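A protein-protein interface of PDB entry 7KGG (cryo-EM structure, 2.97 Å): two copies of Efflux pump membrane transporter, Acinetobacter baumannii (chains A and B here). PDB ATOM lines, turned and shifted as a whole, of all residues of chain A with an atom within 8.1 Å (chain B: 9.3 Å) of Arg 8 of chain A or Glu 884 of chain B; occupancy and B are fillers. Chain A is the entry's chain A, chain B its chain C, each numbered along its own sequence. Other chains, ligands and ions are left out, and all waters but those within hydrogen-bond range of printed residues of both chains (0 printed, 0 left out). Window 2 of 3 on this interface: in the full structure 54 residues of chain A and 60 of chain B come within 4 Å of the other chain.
Arg 8 of chain A touches Glu 884 of chain B. CG1 of Val 10 of chain A touches O of Ala 880 of chain B, 3.6 Å away. Glu 884 of chain B touches Val 10 of chain A (OE1 to CB, 3.6 Å). CG2 of Val 10 of chain A touches NE1 of Trp 886 of chain B (3.96 Å). Phe 11 of chain A touches Ala 881 of chain B. CB of Phe 11 of chain A touches OE2 of Glu 884 of chain B, 3.2 Å away. CG2 of Val 14 of chain A touches O of Leu 877 of chain B, at 3.7 Å. CG2 of Val 14 of chain A touches CH2 of Trp 886 of chain B (3.8 Å).
Of the 17 printed residues of chain A, 4 touch a printed residue of chain B. Printed residues of chain A that touch a printed residue of chain B: Arg 8, Val 10, Phe 11 and Val 14. Hydrophobic or aromatic side chains of chain A within 4 Å of the printed part of chain B: Val 10, Phe 11 and Val 14. Of the 18 printed residues of chain B, 5 touch a printed residue of chain A. Printed residues of chain B that touch a printed residue of chain A: Leu 877, Ala 880, Ala 881, Glu 884 and Trp 886. Hydrophobic or aromatic side chains of chain B that line the printed part of chain A: Trp 886.
No position is printed for both chains.
Arg 7 of chain A touches none of the printed residues of chain B. Of chain B, only Glu 884 comes within 4 Å of Arg 8 of chain A. No residue of chain B comes within 4 Å of Pro 9 of chain A. Val 10 of chain A touches just these residues of chain B: Ala 880, Glu 884 and Trp 886. Of the printed residues of chain B, Val 14 of chain A touches Leu 877 and Trp 886. Of the printed residues of chain A, Ala 880 of chain B touches Val 10. Printed residues of chain A within 4 Å of Ala 881 of chain B: Phe 11. The nearest residue of chain A that does not touch Glu 884 of chain B is Pro 9 of chain A (4.4 Å). The nearest printed residue of chain B that does not touch Phe 11 of chain A is Leu 882 of chain B (5.2 Å).
N of Ser 885 of chain B is in hydrogen-bond range of O of Ala 880 of chain B, at 3.4 Å.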
ATOM      1  N   SER A   2      14.402  -6.164  17.825  1.00  0.00           N
ATOM      2  CA  SER A   2      14.321  -6.300  19.275  1.00  0.00           C
ATOM      3  C   SER A   2      15.418  -7.196  19.834  1.00  0.00           C
ATOM      4  O   SER A   2      15.858  -6.981  20.969  1.00  0.00           O
ATOM      5  CB  SER A   2      12.949  -6.845  19.670  1.00  0.00           C
ATOM      6  OG  SER A   2      11.925  -5.933  19.318  1.00  0.00           O
ATOM      7  N   GLN A   3      15.872  -8.189  19.066  1.00  0.00           N
ATOM      8  CA  GLN A   3      16.965  -9.038  19.530  1.00  0.00           C
ATOM      9  C   GLN A   3      18.207  -8.210  19.828  1.00  0.00           C
ATOM     10  O   GLN A   3      19.007  -8.564  20.700  1.00  0.00           O
ATOM     11  CB  GLN A   3      17.269 -10.111  18.484  1.00  0.00           C
ATOM     12  CG  GLN A   3      18.348 -11.101  18.896  1.00  0.00           C
ATOM     13  CD  GLN A   3      17.965 -11.901  20.126  1.00  0.00           C
ATOM     14  OE1 GLN A   3      18.465 -11.654  21.223  1.00  0.00           O
ATOM     15  NE2 GLN A   3      17.069 -12.865  19.949  1.00  0.00           N
ATOM     16  N   PHE A   4      18.458  -7.113  19.197  1.00  0.00           N
ATOM     17  CA  PHE A   4      19.633  -6.308  19.574  1.00  0.00           C
ATOM     18  C   PHE A   4      19.421  -5.870  21.001  1.00  0.00           C
ATOM     19  O   PHE A   4      20.303  -6.146  21.803  1.00  0.00           O
ATOM     20  CB  PHE A   4      19.804  -5.113  18.659  1.00  0.00           C
ATOM     21  CG  PHE A   4      20.882  -4.142  19.048  1.00  0.00           C
ATOM     22  CD1 PHE A   4      20.677  -3.221  20.059  1.00  0.00           C
ATOM     23  CD2 PHE A   4      22.079  -4.111  18.361  1.00  0.00           C
ATOM     24  CE1 PHE A   4      21.666  -2.315  20.395  1.00  0.00           C
ATOM     25  CE2 PHE A   4      23.069  -3.210  18.707  1.00  0.00           C
ATOM     26  CZ  PHE A   4      22.859  -2.310  19.720  1.00  0.00           C
ATOM     27  N   PHE A   5      18.225  -5.446  21.342  1.00  0.00           N
ATOM     28  CA  PHE A   5      18.055  -4.821  22.647  1.00  0.00           C
ATOM     29  C   PHE A   5      17.826  -5.823  23.770  1.00  0.00           C
ATOM     30  O   PHE A   5      18.055  -5.481  24.936  1.00  0.00           O
ATOM     31  CB  PHE A   5      16.885  -3.839  22.585  1.00  0.00           C
ATOM     32  CG  PHE A   5      17.068  -2.754  21.568  1.00  0.00           C
ATOM     33  CD1 PHE A   5      17.881  -1.665  21.831  1.00  0.00           C
ATOM     34  CD2 PHE A   5      16.446  -2.836  20.334  1.00  0.00           C
ATOM     35  CE1 PHE A   5      18.051  -0.670  20.888  1.00  0.00           C
ATOM     36  CE2 PHE A   5      16.617  -1.847  19.389  1.00  0.00           C
ATOM     37  CZ  PHE A   5      17.420  -0.763  19.666  1.00  0.00           C
ATOM     38  N   ILE A   6      17.377  -7.041  23.459  1.00  0.00           N
ATOM     39  CA  ILE A   6      17.173  -8.036  24.507  1.00  0.00           C
ATOM     40  C   ILE A   6      18.492  -8.366  25.195  1.00  0.00           C
ATOM     41  O   ILE A   6      18.555  -8.479  26.425  1.00  0.00           O
ATOM     42  CB  ILE A   6      16.502  -9.297  23.932  1.00  0.00           C
ATOM     43  CG1 ILE A   6      15.109  -8.957  23.395  1.00  0.00           C
ATOM     44  CG2 ILE A   6      16.415 -10.387  24.995  1.00  0.00           C
ATOM     45  CD1 ILE A   6      14.473 -10.062  22.577  1.00  0.00           C
ATOM     46  N   ARG A   7      19.562  -8.525  24.420  1.00  0.00           N
ATOM     47  CA  ARG A   7      20.875  -8.846  24.959  1.00  0.00           C
ATOM     48  C   ARG A   7      21.639  -7.618  25.435  1.00  0.00           C
ATOM     49  O   ARG A   7      22.715  -7.764  26.020  1.00  0.00           O
ATOM     50  CB  ARG A   7      21.706  -9.587  23.906  1.00  0.00           C
ATOM     51  CG  ARG A   7      21.168 -10.964  23.554  1.00  0.00           C
ATOM     52  CD  ARG A   7      22.018 -11.636  22.489  1.00  0.00           C
ATOM     53  NE  ARG A   7      23.358 -11.950  22.975  1.00  0.00           N
ATOM     54  CZ  ARG A   7      24.351 -12.391  22.208  1.00  0.00           C
ATOM     55  NH1 ARG A   7      25.535 -12.651  22.742  1.00  0.00           N
ATOM     56  NH2 ARG A   7      24.161 -12.575  20.907  1.00  0.00           N
ATOM     57  N   ARG A   8      21.114  -6.417  25.200  1.00  0.00           N
ATOM     58  CA  ARG A   8      21.769  -5.167  25.585  1.00  0.00           C
ATOM     59  C   ARG A   8      20.748  -4.248  26.242  1.00  0.00           C
ATOM     60  O   ARG A   8      20.362  -3.217  25.678  1.00  0.00           O
ATOM     61  CB  ARG A   8      22.417  -4.508  24.367  1.00  0.00           C
ATOM     62  CG  ARG A   8      23.791  -5.071  24.043  1.00  0.00           C
ATOM     63  CD  ARG A   8      24.374  -4.452  22.789  1.00  0.00           C
ATOM     64  NE  ARG A   8      23.970  -5.192  21.593  1.00  0.00           N
ATOM     65  CZ  ARG A   8      24.778  -5.948  20.853  1.00  0.00           C
ATOM     66  NH1 ARG A   8      24.297  -6.573  19.787  1.00  0.00           N
ATOM     67  NH2 ARG A   8      26.059  -6.097  21.168  1.00  0.00           N
ATOM     68  N   PRO A   9      20.284  -4.597  27.445  1.00  0.00           N
ATOM     69  CA  PRO A   9      19.270  -3.756  28.106  1.00  0.00           C
ATOM     70  C   PRO A   9      19.738  -2.337  28.381  1.00  0.00           C
ATOM     71  O   PRO A   9      18.920  -1.409  28.379  1.00  0.00           O
ATOM     72  CB  PRO A   9      18.983  -4.520  29.408  1.00  0.00           C
ATOM     73  CG  PRO A   9      19.442  -5.919  29.143  1.00  0.00           C
ATOM     74  CD  PRO A   9      20.641  -5.762  28.271  1.00  0.00           C
ATOM     75  N   VAL A  10      21.034  -2.145  28.635  1.00  0.00           N
ATOM     76  CA  VAL A  10      21.526  -0.830  29.031  1.00  0.00           C
ATOM     77  C   VAL A  10      21.311   0.184  27.913  1.00  0.00           C
ATOM     78  O   VAL A  10      20.949   1.336  28.169  1.00  0.00           O
ATOM     79  CB  VAL A  10      23.006  -0.915  29.442  1.00  0.00           C
ATOM     80  CG1 VAL A  10      23.588   0.479  29.630  1.00  0.00           C
ATOM     81  CG2 VAL A  10      23.155  -1.734  30.714  1.00  0.00           C
ATOM     82  N   PHE A  11      21.506  -0.211  26.689  1.00  0.00           N
ATOM     83  CA  PHE A  11      21.401   0.687  25.542  1.00  0.00           C
ATOM     84  C   PHE A  11      19.937   1.009  25.319  1.00  0.00           C
ATOM     85  O   PHE A  11      19.753   2.068  24.845  1.00  0.00           O
ATOM     86  CB  PHE A  11      22.069  -0.050  24.386  1.00  0.00           C
ATOM     87  CG  PHE A  11      22.358   0.723  23.125  1.00  0.00           C
ATOM     88  CD1 PHE A  11      21.366   1.371  22.418  1.00  0.00           C
ATOM     89  CD2 PHE A  11      23.640   0.753  22.613  1.00  0.00           C
ATOM     90  CE1 PHE A  11      21.654   2.065  21.256  1.00  0.00           C
ATOM     91  CE2 PHE A  11      23.928   1.448  21.453  1.00  0.00           C
ATOM     92  CZ  PHE A  11      22.934   2.104  20.777  1.00  0.00           C
ATOM     93  N   ALA A  12      18.982   0.127  25.537  1.00  0.00           N
ATOM     94  CA  ALA A  12      17.557   0.431  25.476  1.00  0.00           C
ATOM     95  C   ALA A  12      17.151   1.380  26.596  1.00  0.00           C
ATOM     96  O   ALA A  12      16.381   2.322  26.374  1.00  0.00           O
ATOM     97  CB  ALA A  12      16.743  -0.860  25.547  1.00  0.00           C
ATOM     98  N   TRP A  13      17.658   1.148  27.809  1.00  0.00           N
ATOM     99  CA  TRP A  13      17.380   2.061  28.911  1.00  0.00           C
ATOM    100  C   TRP A  13      17.953   3.447  28.644  1.00  0.00           C
ATOM    101  O   TRP A  13      17.342   4.451  29.022  1.00  0.00           O
ATOM    102  CB  TRP A  13      17.945   1.502  30.217  1.00  0.00           C
ATOM    103  CG  TRP A  13      16.965   0.681  30.998  1.00  0.00           C
ATOM    104  CD1 TRP A  13      17.097  -0.628  31.358  1.00  0.00           C
ATOM    105  CD2 TRP A  13      15.703   1.115  31.520  1.00  0.00           C
ATOM    106  NE1 TRP A  13      15.996  -1.037  32.070  1.00  0.00           N
ATOM    107  CE2 TRP A  13      15.125   0.015  32.184  1.00  0.00           C
ATOM    108  CE3 TRP A  13      15.007   2.327  31.492  1.00  0.00           C
ATOM    109  CZ2 TRP A  13      13.884   0.091  32.811  1.00  0.00           C
ATOM    110  CZ3 TRP A  13      13.775   2.399  32.114  1.00  0.00           C
ATOM    111  CH2 TRP A  13      13.227   1.288  32.766  1.00  0.00           C
ATOM    112  N   VAL A  14      19.125   3.519  28.013  1.00  0.00           N
ATOM    113  CA  VAL A  14      19.734   4.809  27.711  1.00  0.00           C
ATOM    114  C   VAL A  14      18.865   5.589  26.736  1.00  0.00           C
ATOM    115  O   VAL A  14      18.708   6.808  26.864  1.00  0.00           O
ATOM    116  CB  VAL A  14      21.160   4.607  27.167  1.00  0.00           C
ATOM    117  CG1 VAL A  14      21.621   5.834  26.389  1.00  0.00           C
ATOM    118  CG2 VAL A  14      22.121   4.302  28.306  1.00  0.00           C
ATOM    119  N   ILE A  15      18.298   4.907  25.739  1.00  0.00           N
ATOM    120  CA  ILE A  15      17.403   5.596  24.810  1.00  0.00           C
ATOM    121  C   ILE A  15      16.212   6.190  25.556  1.00  0.00           C
ATOM    122  O   ILE A  15      15.838   7.354  25.342  1.00  0.00           O
ATOM    123  CB  ILE A  15      16.946   4.639  23.693  1.00  0.00           C
ATOM    124  CG1 ILE A  15      18.135   4.252  22.809  1.00  0.00           C
ATOM    125  CG2 ILE A  15      15.833   5.283  22.864  1.00  0.00           C
ATOM    126  CD1 ILE A  15      17.803   3.233  21.739  1.00  0.00           C
ATOM    127  N   ILE A 487      11.789  -1.738  21.578  1.00  0.00           N
ATOM    128  CA  ILE A 487      13.131  -1.486  22.091  1.00  0.00           C
ATOM    129  C   ILE A 487      13.147  -1.724  23.595  1.00  0.00           C
ATOM    130  O   ILE A 487      13.903  -2.562  24.097  1.00  0.00           O
ATOM    131  CB  ILE A 487      13.587  -0.054  21.753  1.00  0.00           C
ATOM    132  CG1 ILE A 487      13.716   0.104  20.233  1.00  0.00           C
ATOM    133  CG2 ILE A 487      14.897   0.273  22.473  1.00  0.00           C
ATOM    134  CD1 ILE A 487      14.388   1.387  19.786  1.00  0.00           C
ATOM    135  N   ALA A 491      13.135  -5.652  26.471  1.00  0.00           N
ATOM    136  CA  ALA A 491      14.160  -5.751  27.504  1.00  0.00           C
ATOM    137  C   ALA A 491      13.539  -5.880  28.888  1.00  0.00           C
ATOM    138  O   ALA A 491      13.982  -6.700  29.703  1.00  0.00           O
ATOM    139  CB  ALA A 491      15.085  -4.536  27.440  1.00  0.00           C
ATOM    140  N   THR A 495      13.939  -9.043  31.468  1.00  0.00           N
ATOM    141  CA  THR A 495      14.625  -8.864  32.746  1.00  0.00           C
ATOM    142  C   THR A 495      13.672  -8.859  33.938  1.00  0.00           C
ATOM    143  O   THR A 495      13.780  -9.709  34.827  1.00  0.00           O
ATOM    144  CB  THR A 495      15.437  -7.561  32.722  1.00  0.00           C
ATOM    145  OG1 THR A 495      14.557  -6.448  32.520  1.00  0.00           O
ATOM    146  CG2 THR A 495      16.475  -7.597  31.608  1.00  0.00           C
ATOM    147  N   SER B 440      33.064   1.049  16.429  1.00  0.00           N
ATOM    148  CA  SER B 440      32.094   1.536  17.404  1.00  0.00           C
ATOM    149  C   SER B 440      32.714   2.595  18.311  1.00  0.00           C
ATOM    150  O   SER B 440      32.073   3.620  18.590  1.00  0.00           O
ATOM    151  CB  SER B 440      31.531   0.376  18.228  1.00  0.00           C
ATOM    152  OG  SER B 440      30.802  -0.521  17.408  1.00  0.00           O
ATOM    153  N   PHE B 876      27.822  10.646  30.084  1.00  0.00           N
ATOM    154  CA  PHE B 876      27.665   9.427  30.869  1.00  0.00           C
ATOM    155  C   PHE B 876      26.726   8.451  30.176  1.00  0.00           C
ATOM    156  O   PHE B 876      27.004   7.249  30.107  1.00  0.00           O
ATOM    157  CB  PHE B 876      27.146   9.763  32.267  1.00  0.00           C
ATOM    158  CG  PHE B 876      26.865   8.552  33.111  1.00  0.00           C
ATOM    159  CD1 PHE B 876      27.901   7.820  33.665  1.00  0.00           C
ATOM    160  CD2 PHE B 876      25.563   8.139  33.341  1.00  0.00           C
ATOM    161  CE1 PHE B 876      27.645   6.705  34.437  1.00  0.00           C
ATOM    162  CE2 PHE B 876      25.301   7.025  34.112  1.00  0.00           C
ATOM    163  CZ  PHE B 876      26.343   6.307  34.660  1.00  0.00           C
ATOM    164  N   LEU B 877      25.603   8.951  29.657  1.00  0.00           N
ATOM    165  CA  LEU B 877      24.654   8.075  28.977  1.00  0.00           C
ATOM    166  C   LEU B 877      25.277   7.444  27.737  1.00  0.00           C
ATOM    167  O   LEU B 877      25.120   6.240  27.498  1.00  0.00           O
ATOM    168  CB  LEU B 877      23.398   8.861  28.601  1.00  0.00           C
ATOM    169  CG  LEU B 877      22.396   9.172  29.716  1.00  0.00           C
ATOM    170  CD1 LEU B 877      21.153   9.820  29.131  1.00  0.00           C
ATOM    171  CD2 LEU B 877      22.021   7.924  30.505  1.00  0.00           C
ATOM    172  N   VAL B 878      25.995   8.240  26.941  1.00  0.00           N
ATOM    173  CA  VAL B 878      26.614   7.714  25.729  1.00  0.00           C
ATOM    174  C   VAL B 878      27.657   6.660  26.076  1.00  0.00           C
ATOM    175  O   VAL B 878      27.741   5.611  25.426  1.00  0.00           O
ATOM    176  CB  VAL B 878      27.221   8.861  24.902  1.00  0.00           C
ATOM    177  CG1 VAL B 878      28.129   8.310  23.810  1.00  0.00           C
ATOM    178  CG2 VAL B 878      26.121   9.721  24.300  1.00  0.00           C
ATOM    179  N   LEU B 879      28.478   6.922  27.096  1.00  0.00           N
ATOM    180  CA  LEU B 879      29.507   5.961  27.474  1.00  0.00           C
ATOM    181  C   LEU B 879      28.892   4.684  28.030  1.00  0.00           C
ATOM    182  O   LEU B 879      29.396   3.584  27.773  1.00  0.00           O
ATOM    183  CB  LEU B 879      30.458   6.591  28.491  1.00  0.00           C
ATOM    184  CG  LEU B 879      31.501   7.565  27.935  1.00  0.00           C
ATOM    185  CD1 LEU B 879      32.327   8.147  29.067  1.00  0.00           C
ATOM    186  CD2 LEU B 879      32.402   6.888  26.910  1.00  0.00           C
ATOM    187  N   ALA B 880      27.809   4.803  28.801  1.00  0.00           N
ATOM    188  CA  ALA B 880      27.121   3.614  29.291  1.00  0.00           C
ATOM    189  C   ALA B 880      26.560   2.797  28.137  1.00  0.00           C
ATOM    190  O   ALA B 880      26.634   1.563  28.144  1.00  0.00           O
ATOM    191  CB  ALA B 880      26.006   4.014  30.257  1.00  0.00           C
ATOM    192  N   ALA B 881      25.991   3.470  27.136  1.00  0.00           N
ATOM    193  CA  ALA B 881      25.514   2.766  25.952  1.00  0.00           C
ATOM    194  C   ALA B 881      26.656   2.055  25.236  1.00  0.00           C
ATOM    195  O   ALA B 881      26.516   0.901  24.815  1.00  0.00           O
ATOM    196  CB  ALA B 881      24.821   3.747  25.008  1.00  0.00           C
ATOM    197  N   LEU B 882      27.797   2.733  25.088  1.00  0.00           N
ATOM    198  CA  LEU B 882      28.926   2.142  24.378  1.00  0.00           C
ATOM    199  C   LEU B 882      29.479   0.928  25.117  1.00  0.00           C
ATOM    200  O   LEU B 882      29.759  -0.105  24.500  1.00  0.00           O
ATOM    201  CB  LEU B 882      30.021   3.192  24.179  1.00  0.00           C
ATOM    202  CG  LEU B 882      31.314   2.719  23.509  1.00  0.00           C
ATOM    203  CD1 LEU B 882      31.050   2.255  22.086  1.00  0.00           C
ATOM    204  CD2 LEU B 882      32.356   3.826  23.528  1.00  0.00           C
ATOM    205  N   TYR B 883      29.643   1.033  26.435  1.00  0.00           N
ATOM    206  CA  TYR B 883      30.258  -0.021  27.230  1.00  0.00           C
ATOM    207  C   TYR B 883      29.256  -1.029  27.776  1.00  0.00           C
ATOM    208  O   TYR B 883      29.674  -2.042  28.346  1.00  0.00           O
ATOM    209  CB  TYR B 883      31.036   0.592  28.402  1.00  0.00           C
ATOM    210  CG  TYR B 883      32.246   1.400  27.986  1.00  0.00           C
ATOM    211  CD1 TYR B 883      33.188   0.880  27.108  1.00  0.00           C
ATOM    212  CD2 TYR B 883      32.444   2.684  28.474  1.00  0.00           C
ATOM    213  CE1 TYR B 883      34.292   1.616  26.728  1.00  0.00           C
ATOM    214  CE2 TYR B 883      33.545   3.427  28.100  1.00  0.00           C
ATOM    215  CZ  TYR B 883      34.466   2.889  27.227  1.00  0.00           C
ATOM    216  OH  TYR B 883      35.563   3.628  26.853  1.00  0.00           O
ATOM    217  N   GLU B 884      27.956  -0.785  27.616  1.00  0.00           N
ATOM    218  CA  GLU B 884      26.925  -1.675  28.149  1.00  0.00           C
ATOM    219  C   GLU B 884      27.124  -1.910  29.644  1.00  0.00           C
ATOM    220  O   GLU B 884      26.969  -3.025  30.144  1.00  0.00           O
ATOM    221  CB  GLU B 884      26.903  -3.005  27.392  1.00  0.00           C
ATOM    222  CG  GLU B 884      26.478  -2.881  25.939  1.00  0.00           C
ATOM    223  CD  GLU B 884      25.032  -2.457  25.789  1.00  0.00           C
ATOM    224  OE1 GLU B 884      24.212  -2.819  26.660  1.00  0.00           O
ATOM    225  OE2 GLU B 884      24.713  -1.763  24.801  1.00  0.00           O
ATOM    226  N   SER B 885      27.470  -0.845  30.366  1.00  0.00           N
ATOM    227  CA  SER B 885      27.692  -0.928  31.800  1.00  0.00           C
ATOM    228  C   SER B 885      27.358   0.415  32.430  1.00  0.00           C
ATOM    229  O   SER B 885      27.590   1.471  31.833  1.00  0.00           O
ATOM    230  CB  SER B 885      29.137  -1.324  32.126  1.00  0.00           C
ATOM    231  OG  SER B 885      29.334  -1.426  33.525  1.00  0.00           O
ATOM    232  N   TRP B 886      26.811   0.365  33.642  1.00  0.00           N
ATOM    233  CA  TRP B 886      26.408   1.566  34.360  1.00  0.00           C
ATOM    234  C   TRP B 886      27.533   2.181  35.181  1.00  0.00           C
ATOM    235  O   TRP B 886      27.359   3.287  35.705  1.00  0.00           O
ATOM    236  CB  TRP B 886      25.227   1.253  35.285  1.00  0.00           C
ATOM    237  CG  TRP B 886      23.907   1.137  34.579  1.00  0.00           C
ATOM    238  CD1 TRP B 886      23.039   0.086  34.635  1.00  0.00           C
ATOM    239  CD2 TRP B 886      23.301   2.111  33.719  1.00  0.00           C
ATOM    240  NE1 TRP B 886      21.934   0.342  33.862  1.00  0.00           N
ATOM    241  CE2 TRP B 886      22.070   1.578  33.289  1.00  0.00           C
ATOM    242  CE3 TRP B 886      23.680   3.380  33.270  1.00  0.00           C
ATOM    243  CZ2 TRP B 886      21.216   2.269  32.431  1.00  0.00           C
ATOM    244  CZ3 TRP B 886      22.831   4.064  32.419  1.00  0.00           C
ATOM    245  CH2 TRP B 886      21.614   3.507  32.008  1.00  0.00           C
ATOM    246  N   ALA B 887      28.673   1.504  35.308  1.00  0.00           N
ATOM    247  CA  ALA B 887      29.775   1.961  36.148  1.00  0.00           C
ATOM    248  C   ALA B 887      31.069   2.188  35.386  1.00  0.00           C
ATOM    249  O   ALA B 887      31.858   3.055  35.768  1.00  0.00           O
ATOM    250  CB  ALA B 887      30.029   0.948  37.269  1.00  0.00           C
ATOM    251  N   ILE B 888      31.312   1.430  34.321  1.00  0.00           N
ATOM    252  CA  ILE B 888      32.525   1.564  33.519  1.00  0.00           C
ATOM    253  C   ILE B 888      32.683   3.004  33.040  1.00  0.00           C
ATOM    254  O   ILE B 888      33.810   3.520  33.022  1.00  0.00           O
ATOM    255  CB  ILE B 888      32.514   0.581  32.336  1.00  0.00           C
ATOM    256  CG1 ILE B 888      32.640  -0.854  32.860  1.00  0.00           C
ATOM    257  CG2 ILE B 888      33.641   0.912  31.352  1.00  0.00           C
ATOM    258  CD1 ILE B 888      32.846  -1.908  31.787  1.00  0.00           C
ATOM    259  N   PRO B 889      31.609   3.691  32.634  1.00  0.00           N
ATOM    260  CA  PRO B 889      31.780   5.064  32.130  1.00  0.00           C
ATOM    261  C   PRO B 889      32.489   5.999  33.096  1.00  0.00           C
ATOM    262  O   PRO B 889      33.186   6.917  32.646  1.00  0.00           O
ATOM    263  CB  PRO B 889      30.337   5.515  31.873  1.00  0.00           C
ATOM    264  CG  PRO B 889      29.617   4.264  31.552  1.00  0.00           C
ATOM    265  CD  PRO B 889      30.230   3.210  32.428  1.00  0.00           C
ATOM    266  N   GLU B 938      38.214   0.802  26.287  1.00  0.00           N
ATOM    267  CA  GLU B 938      37.652  -0.166  25.352  1.00  0.00           C
ATOM    268  C   GLU B 938      38.588  -1.355  25.176  1.00  0.00           C
ATOM    269  O   GLU B 938      38.155  -2.512  25.223  1.00  0.00           O
ATOM    270  CB  GLU B 938      37.374   0.508  24.008  1.00  0.00           C
ATOM    271  CG  GLU B 938      36.824  -0.424  22.935  1.00  0.00           C
ATOM    272  CD  GLU B 938      35.338  -0.678  23.090  1.00  0.00           C
ATOM    273  OE1 GLU B 938      34.940  -1.859  23.163  1.00  0.00           O
ATOM    274  OE2 GLU B 938      34.568   0.304  23.139  1.00  0.00           O
ATOM    275  N   LYS B 941      38.584  -3.602  28.343  1.00  0.00           N
ATOM    276  CA  LYS B 941      37.371  -4.436  28.443  1.00  0.00           C
ATOM    277  C   LYS B 941      37.410  -5.480  27.340  1.00  0.00           C
ATOM    278  O   LYS B 941      37.027  -6.484  27.656  1.00  0.00           O
ATOM    279  CB  LYS B 941      36.114  -3.585  28.361  1.00  0.00           C
ATOM    280  CG  LYS B 941      34.788  -4.319  28.227  1.00  0.00           C
ATOM    281  CD  LYS B 941      33.627  -3.406  27.920  1.00  0.00           C
ATOM    282  CE  LYS B 941      32.879  -3.843  26.681  1.00  0.00           C
ATOM    283  NZ  LYS B 941      31.410  -3.705  26.811  1.00  0.00           N
ATOM    284  N   GLU B 945      37.433  -9.548  28.309  1.00  0.00           N
ATOM    285  CA  GLU B 945      36.440 -10.493  27.812  1.00  0.00           C
ATOM    286  C   GLU B 945      37.074 -11.712  27.152  1.00  0.00           C
ATOM    287  O   GLU B 945      36.376 -12.704  26.916  1.00  0.00           O
ATOM    288  CB  GLU B 945      35.503  -9.804  26.819  1.00  0.00           C
ATOM    289  CG  GLU B 945      34.610  -8.744  27.442  1.00  0.00           C
ATOM    290  CD  GLU B 945      33.710  -8.072  26.424  1.00  0.00           C
ATOM    291  OE1 GLU B 945      33.869  -8.343  25.216  1.00  0.00           O
ATOM    292  OE2 GLU B 945      32.841  -7.274  26.832  1.00  0.00           O
